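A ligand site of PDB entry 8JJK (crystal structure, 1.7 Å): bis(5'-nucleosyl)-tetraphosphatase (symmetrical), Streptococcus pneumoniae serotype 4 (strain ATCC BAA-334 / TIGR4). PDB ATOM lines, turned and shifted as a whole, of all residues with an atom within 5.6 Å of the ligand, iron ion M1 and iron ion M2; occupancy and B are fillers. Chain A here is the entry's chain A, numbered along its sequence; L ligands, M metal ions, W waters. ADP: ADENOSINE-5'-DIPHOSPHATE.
OD2 of Asp 59 sits close to NH1 of Arg 26.
The side-chain carboxylate (OD2) of Asp 135 lies within salt-bridge range of the guanidinium group (NH2) of Arg 141 (3.97 Å).
NE2 of His 117 lies close to OG1 of Thr 118 (3.2 Å).
ND1 of His 91 sits at hydrogen-bond distance from O of Asn 88.
The side-chain hydroxyl (OG1) of Thr 168 lies within hydrogen-bond range of the backbone carbonyl oxygen (O) of Glu 164, at 2.9 Å.
Water W1 lies within hydrogen-bond range of the side-chain carboxylate of Asp 135 (2.6 Å) and an oxygen (O3A) of the ligand (2.9 Å).
Water W8 lies within hydrogen-bond range of a nitrogen (N7) of the ligand (2.5 Å), the backbone carbonyl oxygen (O) of Thr 118 (2.8 Å) and the side-chain hydroxyl (OG1) of Thr 183 (2.8 Å).
Water W6 lies within hydrogen-bond range of O1B of the ligand (2.7 Å), NH2 of Arg 26 (3.4 Å) and NH1 of Arg 141 (3.4 Å).
Water W4 lies within hydrogen-bond range of OD2 of Asp 135 (3.1 Å), NH2 of Arg 141 (3.2 Å) and O1A of the ligand (3.2 Å).
Water W3 lies within hydrogen-bond range of O3' of the ligand and ND2 of Asn 88.
The side-chain hydroxyl (OG1) of Thr 183 lies within hydrogen-bond range of a nitrogen (N6) of the ligand, at 2.7 Å.
The side-chain hydroxyl (OG1) of Thr 118 sits close to an oxygen (O2A) of the ligand (2.8 Å).
An oxygen (O1B) of the ligand is in salt-bridge range of the side-chain amino group (NZ) of Lys 62, 3.2 Å away.
The guanidinium group (NH2) of Arg 141 sits close to an oxygen (O3B) of the ligand (2.9 Å).
An oxygen (O1B) of the ligand is in salt-bridge range of the guanidinium group (NH1) of Arg 26 (3.6 Å).
The backbone NH (N) of Tyr 180 sits at hydrogen-bond distance from a nitrogen (N1) of the ligand (3.0 Å).
O of Tyr 180 lies close to N6 of the ligand, 3.5 Å away.
N3 of the ligand is in hydrogen-bond range of ND2 of Asn 88 (3.4 Å).
Thr 118 touches iron ion M2 (OG1 to FE, 3.8 Å).
Of the 23 residues printed, 4 come within 4 Å of iron ion M2.
Iron ion M1 is bound by water W1 (2.0 Å), a ring nitrogen (NE2) of His 29 (2.1 Å), the side-chain carboxylate of Asp 135 (2.1 Å), an oxygen (O3B) of the ligand (2.2 Å), a ring nitrogen (NE2) of His 58 (2.2 Å) and the side-chain carboxylate of Asp 59 (2.2 Å).
Iron ion M1 has six donor atoms within binding distance.
Residues that only touch iron ion M1: Arg 26 and Arg 141.
Six residues have an atom within 4 Å of iron ion M1: Arg 26, His 29, His 58, Asp 59, Asp 135 and Arg 141.
Residues that only touch the ligand: Thr 168 (3.7 Å), Leu 172 (3.5 Å), Pro 178 (3.5 Å) and Ile 179 (3.7 Å).
Hydrophobic or aromatic side chains within 4 Å of the ligand: His 29, His 91, His 117, Leu 172, Ile 179 and Tyr 180.
16 residues have an atom within 4 Å of the ligand: Arg 26, His 29, Asp 59, Lys 62, Asn 88, His 91, His 117, Thr 118, Asp 135, Arg 141, Thr 168, Leu 172, Pro 178, Ile 179, Tyr 180 and Thr 183.
Along chain A the residues within 4 Å of the ligand span positions 26 to 183.
Iron ion M2 is bound by water W1 (2.0 Å), OD1 of Asp 59 (2.1 Å), O2B of the ligand (2.1 Å), O2A of the ligand (2.1 Å), NE2 of His 117 (2.2 Å) and NE2 of His 91 (2.2 Å).
Iron ion M2 has six donor atoms within binding distance.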
ATOM      1  N   ARG A  26      15.310  19.507 -18.632  1.00  0.00           N
ATOM      2  CA  ARG A  26      15.760  18.148 -18.887  1.00  0.00           C
ATOM      3  C   ARG A  26      17.249  17.967 -18.541  1.00  0.00           C
ATOM      4  O   ARG A  26      17.627  16.948 -17.970  1.00  0.00           O
ATOM      5  CB  ARG A  26      15.453  17.728 -20.331  1.00  0.00           C
ATOM      6  CG  ARG A  26      15.786  16.275 -20.668  1.00  0.00           C
ATOM      7  CD  ARG A  26      15.085  15.276 -19.759  1.00  0.00           C
ATOM      8  NE  ARG A  26      13.636  15.467 -19.778  1.00  0.00           N
ATOM      9  CZ  ARG A  26      12.773  14.780 -19.026  1.00  0.00           C
ATOM     10  NH1 ARG A  26      13.199  13.830 -18.200  1.00  0.00           N
ATOM     11  NH2 ARG A  26      11.474  15.032 -19.110  1.00  0.00           N
ATOM     12  N   HIS A  29      17.615  17.847 -14.853  1.00  0.00           N
ATOM     13  CA  HIS A  29      17.227  16.491 -14.448  1.00  0.00           C
ATOM     14  C   HIS A  29      18.388  15.519 -14.623  1.00  0.00           C
ATOM     15  O   HIS A  29      18.682  14.723 -13.725  1.00  0.00           O
ATOM     16  CB  HIS A  29      15.999  16.032 -15.238  1.00  0.00           C
ATOM     17  CG  HIS A  29      15.739  14.556 -15.193  1.00  0.00           C
ATOM     18  ND1 HIS A  29      15.341  13.906 -14.040  1.00  0.00           N
ATOM     19  CD2 HIS A  29      15.797  13.602 -16.155  1.00  0.00           C
ATOM     20  CE1 HIS A  29      15.160  12.622 -14.302  1.00  0.00           C
ATOM     21  NE2 HIS A  29      15.421  12.420 -15.578  1.00  0.00           N
ATOM     22  N   VAL A  33      20.263  13.223 -11.904  1.00  0.00           N
ATOM     23  CA  VAL A  33      20.422  11.757 -11.974  1.00  0.00           C
ATOM     24  C   VAL A  33      21.902  11.371 -11.858  1.00  0.00           C
ATOM     25  O   VAL A  33      22.235  10.378 -11.232  1.00  0.00           O
ATOM     26  CB  VAL A  33      19.749  11.166 -13.243  1.00  0.00           C
ATOM     27  CG1 VAL A  33      19.918   9.657 -13.324  1.00  0.00           C
ATOM     28  CG2 VAL A  33      18.272  11.529 -13.254  1.00  0.00           C
ATOM     29  N   HIS A  58      21.384   9.277 -19.430  1.00  0.00           N
ATOM     30  CA  HIS A  58      20.251   8.361 -19.577  1.00  0.00           C
ATOM     31  C   HIS A  58      19.144   8.936 -20.492  1.00  0.00           C
ATOM     32  O   HIS A  58      18.522   8.194 -21.245  1.00  0.00           O
ATOM     33  CB  HIS A  58      19.701   7.926 -18.207  1.00  0.00           C
ATOM     34  CG  HIS A  58      18.813   8.944 -17.584  1.00  0.00           C
ATOM     35  ND1 HIS A  58      19.283  10.132 -17.075  1.00  0.00           N
ATOM     36  CD2 HIS A  58      17.472   8.977 -17.435  1.00  0.00           C
ATOM     37  CE1 HIS A  58      18.264  10.851 -16.628  1.00  0.00           C
ATOM     38  NE2 HIS A  58      17.154  10.163 -16.825  1.00  0.00           N
ATOM     39  N   ASP A  59      18.941  10.255 -20.422  1.00  0.00           N
ATOM     40  CA  ASP A  59      17.892  10.949 -21.189  1.00  0.00           C
ATOM     41  C   ASP A  59      18.458  11.756 -22.357  1.00  0.00           C
ATOM     42  O   ASP A  59      17.785  12.667 -22.870  1.00  0.00           O
ATOM     43  CB  ASP A  59      17.037  11.848 -20.281  1.00  0.00           C
ATOM     44  CG  ASP A  59      15.855  11.113 -19.627  1.00  0.00           C
ATOM     45  OD1 ASP A  59      15.504   9.980 -20.042  1.00  0.00           O
ATOM     46  OD2 ASP A  59      15.275  11.695 -18.690  1.00  0.00           O
ATOM     47  N   LYS A  62      16.188  12.080 -25.382  1.00  0.00           N
ATOM     48  CA  LYS A  62      14.803  12.418 -25.044  1.00  0.00           C
ATOM     49  C   LYS A  62      14.081  13.219 -26.132  1.00  0.00           C
ATOM     50  O   LYS A  62      12.877  13.046 -26.327  1.00  0.00           O
ATOM     51  CB  LYS A  62      14.742  13.174 -23.705  1.00  0.00           C
ATOM     52  CG  LYS A  62      13.347  13.385 -23.116  1.00  0.00           C
ATOM     53  CD  LYS A  62      12.718  12.105 -22.561  1.00  0.00           C
ATOM     54  CE  LYS A  62      11.419  12.445 -21.828  1.00  0.00           C
ATOM     55  NZ  LYS A  62      10.798  11.291 -21.116  1.00  0.00           N
ATOM     56  N   TRP A  85       5.148   1.727 -30.698  1.00  0.00           N
ATOM     57  CA  TRP A  85       5.213   2.514 -29.471  1.00  0.00           C
ATOM     58  C   TRP A  85       5.654   3.947 -29.768  1.00  0.00           C
ATOM     59  O   TRP A  85       5.345   4.469 -30.845  1.00  0.00           O
ATOM     60  CB  TRP A  85       6.093   1.781 -28.452  1.00  0.00           C
ATOM     61  CG  TRP A  85       5.530   0.422 -28.197  1.00  0.00           C
ATOM     62  CD1 TRP A  85       5.767  -0.724 -28.929  1.00  0.00           C
ATOM     63  CD2 TRP A  85       4.575   0.060 -27.214  1.00  0.00           C
ATOM     64  NE1 TRP A  85       5.029  -1.765 -28.437  1.00  0.00           N
ATOM     65  CE2 TRP A  85       4.292  -1.315 -27.382  1.00  0.00           C
ATOM     66  CE3 TRP A  85       3.940   0.768 -26.175  1.00  0.00           C
ATOM     67  CZ2 TRP A  85       3.401  -2.008 -26.548  1.00  0.00           C
ATOM     68  CZ3 TRP A  85       3.056   0.082 -25.344  1.00  0.00           C
ATOM     69  CH2 TRP A  85       2.780  -1.287 -25.546  1.00  0.00           C
ATOM     70  N   ASN A  88       8.444   7.392 -25.112  1.00  0.00           N
ATOM     71  CA  ASN A  88       8.621   6.786 -23.778  1.00  0.00           C
ATOM     72  C   ASN A  88       9.474   5.534 -23.834  1.00  0.00           C
ATOM     73  O   ASN A  88      10.438   5.399 -23.073  1.00  0.00           O
ATOM     74  CB  ASN A  88       7.275   6.445 -23.117  1.00  0.00           C
ATOM     75  CG  ASN A  88       6.492   7.658 -22.695  1.00  0.00           C
ATOM     76  OD1 ASN A  88       6.987   8.793 -22.711  1.00  0.00           O
ATOM     77  ND2 ASN A  88       5.247   7.428 -22.292  1.00  0.00           N
ATOM     78  N   VAL A  89       9.121   4.618 -24.743  1.00  0.00           N
ATOM     79  CA  VAL A  89       9.881   3.401 -24.955  1.00  0.00           C
ATOM     80  C   VAL A  89      11.183   3.710 -25.703  1.00  0.00           C
ATOM     81  O   VAL A  89      12.252   3.212 -25.315  1.00  0.00           O
ATOM     82  CB  VAL A  89       9.054   2.319 -25.698  1.00  0.00           C
ATOM     83  CG1 VAL A  89       9.890   1.087 -26.005  1.00  0.00           C
ATOM     84  CG2 VAL A  89       7.814   1.913 -24.889  1.00  0.00           C
ATOM     85  N   HIS A  91      13.273   6.381 -26.233  1.00  0.00           N
ATOM     86  CA  HIS A  91      14.407   7.275 -25.922  1.00  0.00           C
ATOM     87  C   HIS A  91      15.534   6.528 -25.208  1.00  0.00           C
ATOM     88  O   HIS A  91      16.701   6.853 -25.382  1.00  0.00           O
ATOM     89  CB  HIS A  91      13.971   8.576 -25.238  1.00  0.00           C
ATOM     90  CG  HIS A  91      13.588   8.411 -23.796  1.00  0.00           C
ATOM     91  ND1 HIS A  91      12.364   7.925 -23.412  1.00  0.00           N
ATOM     92  CD2 HIS A  91      14.252   8.717 -22.659  1.00  0.00           C
ATOM     93  CE1 HIS A  91      12.294   7.908 -22.088  1.00  0.00           C
ATOM     94  NE2 HIS A  91      13.423   8.386 -21.614  1.00  0.00           N
ATOM     95  N   HIS A 117      16.386   2.033 -18.756  1.00  0.00           N
ATOM     96  CA  HIS A 117      16.140   2.953 -17.623  1.00  0.00           C
ATOM     97  C   HIS A 117      14.666   3.310 -17.437  1.00  0.00           C
ATOM     98  O   HIS A 117      14.253   3.703 -16.344  1.00  0.00           O
ATOM     99  CB  HIS A 117      16.983   4.222 -17.723  1.00  0.00           C
ATOM    100  CG  HIS A 117      16.388   5.266 -18.609  1.00  0.00           C
ATOM    101  ND1 HIS A 117      16.742   5.416 -19.928  1.00  0.00           N
ATOM    102  CD2 HIS A 117      15.441   6.218 -18.375  1.00  0.00           C
ATOM    103  CE1 HIS A 117      16.058   6.409 -20.470  1.00  0.00           C
ATOM    104  NE2 HIS A 117      15.259   6.912 -19.538  1.00  0.00           N
ATOM    105  N   THR A 118      13.873   3.172 -18.499  1.00  0.00           N
ATOM    106  CA  THR A 118      12.439   3.460 -18.438  1.00  0.00           C
ATOM    107  C   THR A 118      11.619   2.222 -18.058  1.00  0.00           C
ATOM    108  O   THR A 118      10.771   2.279 -17.163  1.00  0.00           O
ATOM    109  CB  THR A 118      11.930   3.996 -19.793  1.00  0.00           C
ATOM    110  OG1 THR A 118      12.736   5.098 -20.212  1.00  0.00           O
ATOM    111  CG2 THR A 118      10.457   4.413 -19.716  1.00  0.00           C
ATOM    112  N   VAL A 119      11.875   1.123 -18.748  1.00  0.00           N
ATOM    113  CA  VAL A 119      11.024  -0.070 -18.653  1.00  0.00           C
ATOM    114  C   VAL A 119      11.581  -1.181 -17.769  1.00  0.00           C
ATOM    115  O   VAL A 119      10.862  -2.122 -17.417  1.00  0.00           O
ATOM    116  CB  VAL A 119      10.714  -0.643 -20.066  1.00  0.00           C
ATOM    117  CG1 VAL A 119       9.942   0.385 -20.901  1.00  0.00           C
ATOM    118  CG2 VAL A 119      11.992  -1.070 -20.784  1.00  0.00           C
ATOM    119  N   ASP A 135      16.875   7.858 -11.510  1.00  0.00           N
ATOM    120  CA  ASP A 135      16.009   8.613 -12.403  1.00  0.00           C
ATOM    121  C   ASP A 135      14.750   9.097 -11.653  1.00  0.00           C
ATOM    122  O   ASP A 135      14.254  10.227 -11.862  1.00  0.00           O
ATOM    123  CB  ASP A 135      15.616   7.703 -13.576  1.00  0.00           C
ATOM    124  CG  ASP A 135      14.824   8.403 -14.648  1.00  0.00           C
ATOM    125  OD1 ASP A 135      14.955   9.639 -14.835  1.00  0.00           O
ATOM    126  OD2 ASP A 135      14.083   7.669 -15.340  1.00  0.00           O
ATOM    127  N   ARG A 141      13.024  16.014  -8.653  1.00  0.00           N
ATOM    128  CA  ARG A 141      11.695  15.373  -8.719  1.00  0.00           C
ATOM    129  C   ARG A 141      10.865  15.760  -7.498  1.00  0.00           C
ATOM    130  O   ARG A 141      11.400  15.852  -6.389  1.00  0.00           O
ATOM    131  CB  ARG A 141      11.829  13.854  -8.828  1.00  0.00           C
ATOM    132  CG  ARG A 141      12.418  13.338 -10.141  1.00  0.00           C
ATOM    133  CD  ARG A 141      11.336  13.054 -11.181  1.00  0.00           C
ATOM    134  NE  ARG A 141      11.753  11.957 -12.042  1.00  0.00           N
ATOM    135  CZ  ARG A 141      11.785  11.975 -13.372  1.00  0.00           C
ATOM    136  NH1 ARG A 141      11.372  13.054 -14.059  1.00  0.00           N
ATOM    137  NH2 ARG A 141      12.206  10.905 -14.024  1.00  0.00           N
ATOM    138  N   GLU A 164       9.095   1.664  -7.406  1.00  0.00           N
ATOM    139  CA  GLU A 164       8.982   2.489  -8.616  1.00  0.00           C
ATOM    140  C   GLU A 164       8.141   1.802  -9.685  1.00  0.00           C
ATOM    141  O   GLU A 164       7.279   2.436 -10.323  1.00  0.00           O
ATOM    142  CB  GLU A 164      10.361   2.852  -9.170  1.00  0.00           C
ATOM    143  CG  GLU A 164      10.270   3.621 -10.481  1.00  0.00           C
ATOM    144  CD  GLU A 164      11.616   3.997 -11.099  1.00  0.00           C
ATOM    145  OE1 GLU A 164      12.664   3.825 -10.436  1.00  0.00           O
ATOM    146  OE2 GLU A 164      11.612   4.467 -12.249  1.00  0.00           O
ATOM    147  N   THR A 168       4.531   2.952 -11.239  1.00  0.00           N
ATOM    148  CA  THR A 168       4.439   3.253 -12.658  1.00  0.00           C
ATOM    149  C   THR A 168       3.328   2.472 -13.339  1.00  0.00           C
ATOM    150  O   THR A 168       2.537   3.062 -14.108  1.00  0.00           O
ATOM    151  CB  THR A 168       5.794   3.057 -13.318  1.00  0.00           C
ATOM    152  OG1 THR A 168       6.689   4.015 -12.734  1.00  0.00           O
ATOM    153  CG2 THR A 168       5.710   3.275 -14.835  1.00  0.00           C
ATOM    154  N   LEU A 172       0.113   4.318 -14.938  1.00  0.00           N
ATOM    155  CA  LEU A 172      -0.234   4.144 -16.363  1.00  0.00           C
ATOM    156  C   LEU A 172      -1.661   3.634 -16.516  1.00  0.00           C
ATOM    157  O   LEU A 172      -2.425   4.144 -17.342  1.00  0.00           O
ATOM    158  CB  LEU A 172       0.793   3.259 -17.072  1.00  0.00           C
ATOM    159  CG  LEU A 172       2.188   3.878 -17.223  1.00  0.00           C
ATOM    160  CD1 LEU A 172       3.118   2.805 -17.764  1.00  0.00           C
ATOM    161  CD2 LEU A 172       2.209   5.110 -18.116  1.00  0.00           C
ATOM    162  N   PRO A 178      -1.220   2.809 -22.692  1.00  0.00           N
ATOM    163  CA  PRO A 178      -0.653   1.486 -22.975  1.00  0.00           C
ATOM    164  C   PRO A 178       0.594   1.249 -22.138  1.00  0.00           C
ATOM    165  O   PRO A 178       1.344   2.208 -21.847  1.00  0.00           O
ATOM    166  CB  PRO A 178      -0.277   1.566 -24.458  1.00  0.00           C
ATOM    167  CG  PRO A 178      -1.080   2.680 -25.027  1.00  0.00           C
ATOM    168  CD  PRO A 178      -1.358   3.638 -23.905  1.00  0.00           C
ATOM    169  N   ILE A 179       0.811  -0.006 -21.734  1.00  0.00           N
ATOM    170  CA  ILE A 179       1.942  -0.399 -20.901  1.00  0.00           C
ATOM    171  C   ILE A 179       2.851  -1.328 -21.714  1.00  0.00           C
ATOM    172  O   ILE A 179       2.453  -2.426 -22.084  1.00  0.00           O
ATOM    173  CB  ILE A 179       1.485  -1.073 -19.584  1.00  0.00           C
ATOM    174  CG1 ILE A 179       0.672  -0.067 -18.762  1.00  0.00           C
ATOM    175  CG2 ILE A 179       2.683  -1.616 -18.789  1.00  0.00           C
ATOM    176  CD1 ILE A 179      -0.167  -0.674 -17.656  1.00  0.00           C
ATOM    177  N   TYR A 180       4.074  -0.868 -21.977  1.00  0.00           N
ATOM    178  CA  TYR A 180       5.041  -1.684 -22.715  1.00  0.00           C
ATOM    179  C   TYR A 180       5.278  -2.984 -21.955  1.00  0.00           C
ATOM    180  O   TYR A 180       5.485  -2.960 -20.741  1.00  0.00           O
ATOM    181  CB  TYR A 180       6.339  -0.901 -22.941  1.00  0.00           C
ATOM    182  CG  TYR A 180       7.281  -1.595 -23.884  1.00  0.00           C
ATOM    183  CD1 TYR A 180       6.981  -1.690 -25.238  1.00  0.00           C
ATOM    184  CD2 TYR A 180       8.473  -2.153 -23.422  1.00  0.00           C
ATOM    185  CE1 TYR A 180       7.839  -2.338 -26.124  1.00  0.00           C
ATOM    186  CE2 TYR A 180       9.350  -2.789 -24.308  1.00  0.00           C
ATOM    187  CZ  TYR A 180       9.029  -2.875 -25.652  1.00  0.00           C
ATOM    188  OH  TYR A 180       9.889  -3.509 -26.505  1.00  0.00           O
ATOM    189  N   PRO A 181       5.156  -4.137 -22.631  1.00  0.00           N
ATOM    190  CA  PRO A 181       5.164  -5.399 -21.894  1.00  0.00           C
ATOM    191  C   PRO A 181       6.419  -5.659 -21.060  1.00  0.00           C
ATOM    192  O   PRO A 181       6.318  -6.320 -20.026  1.00  0.00           O
ATOM    193  CB  PRO A 181       4.966  -6.448 -22.992  1.00  0.00           C
ATOM    194  CG  PRO A 181       4.084  -5.726 -23.953  1.00  0.00           C
ATOM    195  CD  PRO A 181       4.694  -4.344 -24.015  1.00  0.00           C
ATOM    196  N   THR A 183       7.875  -3.716 -19.104  1.00  0.00           N
ATOM    197  CA  THR A 183       7.592  -3.193 -17.769  1.00  0.00           C
ATOM    198  C   THR A 183       6.915  -4.217 -16.866  1.00  0.00           C
ATOM    199  O   THR A 183       7.212  -4.284 -15.674  1.00  0.00           O
ATOM    200  CB  THR A 183       6.785  -1.895 -17.857  1.00  0.00           C
ATOM    201  OG1 THR A 183       7.639  -0.883 -18.372  1.00  0.00           O
ATOM    202  CG2 THR A 183       6.262  -1.430 -16.498  1.00  0.00           C
HETATM  203  PB  ADP L   1      11.948  10.550 -17.840  1.00  0.00           P
HETATM  204  O1B ADP L   1      10.649  11.317 -17.928  1.00  0.00           O
HETATM  205  O2B ADP L   1      12.601  10.244 -19.192  1.00  0.00           O
HETATM  206  O3B ADP L   1      12.884  11.223 -16.855  1.00  0.00           O
HETATM  207  PA  ADP L   1      11.333   7.671 -17.744  1.00  0.00           P
HETATM  208  O1A ADP L   1      11.377   6.666 -16.623  1.00  0.00           O
HETATM  209  O2A ADP L   1      12.252   7.486 -18.917  1.00  0.00           O
HETATM  210  O3A ADP L   1      11.480   9.163 -17.121  1.00  0.00           O
HETATM  211  O5' ADP L   1       9.814   7.692 -18.239  1.00  0.00           O
HETATM  212  C5' ADP L   1       9.368   8.420 -19.379  1.00  0.00           C
HETATM  213  C4' ADP L   1       7.856   8.214 -19.446  1.00  0.00           C
HETATM  214  O4' ADP L   1       7.626   6.865 -19.844  1.00  0.00           O
HETATM  215  C3' ADP L   1       7.110   8.423 -18.113  1.00  0.00           C
HETATM  216  O3' ADP L   1       5.981   9.279 -18.347  1.00  0.00           O
HETATM  217  C2' ADP L   1       6.664   7.023 -17.697  1.00  0.00           C
HETATM  218  O2' ADP L   1       5.407   6.946 -17.006  1.00  0.00           O
HETATM  219  C1' ADP L   1       6.565   6.320 -19.048  1.00  0.00           C
HETATM  220  N9  ADP L   1       6.596   4.844 -18.967  1.00  0.00           N
HETATM  221  C8  ADP L   1       7.238   4.081 -18.062  1.00  0.00           C
HETATM  222  N7  ADP L   1       7.040   2.766 -18.304  1.00  0.00           N
HETATM  223  C5  ADP L   1       6.238   2.704 -19.372  1.00  0.00           C
HETATM  224  C6  ADP L   1       5.594   1.646 -20.169  1.00  0.00           C
HETATM  225  N6  ADP L   1       5.794   0.376 -19.854  1.00  0.00           N
HETATM  226  N1  ADP L   1       4.815   1.987 -21.220  1.00  0.00           N
HETATM  227  C2  ADP L   1       4.612   3.273 -21.538  1.00  0.00           C
HETATM  228  N3  ADP L   1       5.152   4.314 -20.880  1.00  0.00           N
HETATM  229  C4  ADP L   1       5.948   4.068 -19.809  1.00  0.00           C
HETATM  230 FE    FE M   1      15.007  10.660 -16.711  1.00  0.00          FE
HETATM  231 FE    FE M   2      13.955   8.659 -19.504  1.00  0.00          FE
HETATM  232 MG    MG M   3      13.010   5.156 -14.524  1.00  0.00          MG
HETATM  233  O   HOH W   1      14.358   9.011 -17.556  1.00  0.00           O
HETATM  234  O   HOH W   2       9.314   5.478 -15.850  1.00  0.00           O
HETATM  235  O   HOH W   3       3.140   8.425 -19.775  1.00  0.00           O
HETATM  236  O   HOH W   4      11.513   7.805 -13.588  1.00  0.00           O
HETATM  237  O   HOH W   5       8.903  10.514 -15.996  1.00  0.00           O
HETATM  238  O   HOH W   6       9.553  13.476 -16.848  1.00  0.00           O
HETATM  239  O   HOH W   7       2.060   4.492 -22.940  1.00  0.00           O
HETATM  240  O   HOH W   8       8.257   1.259 -16.697  1.00  0.00           O
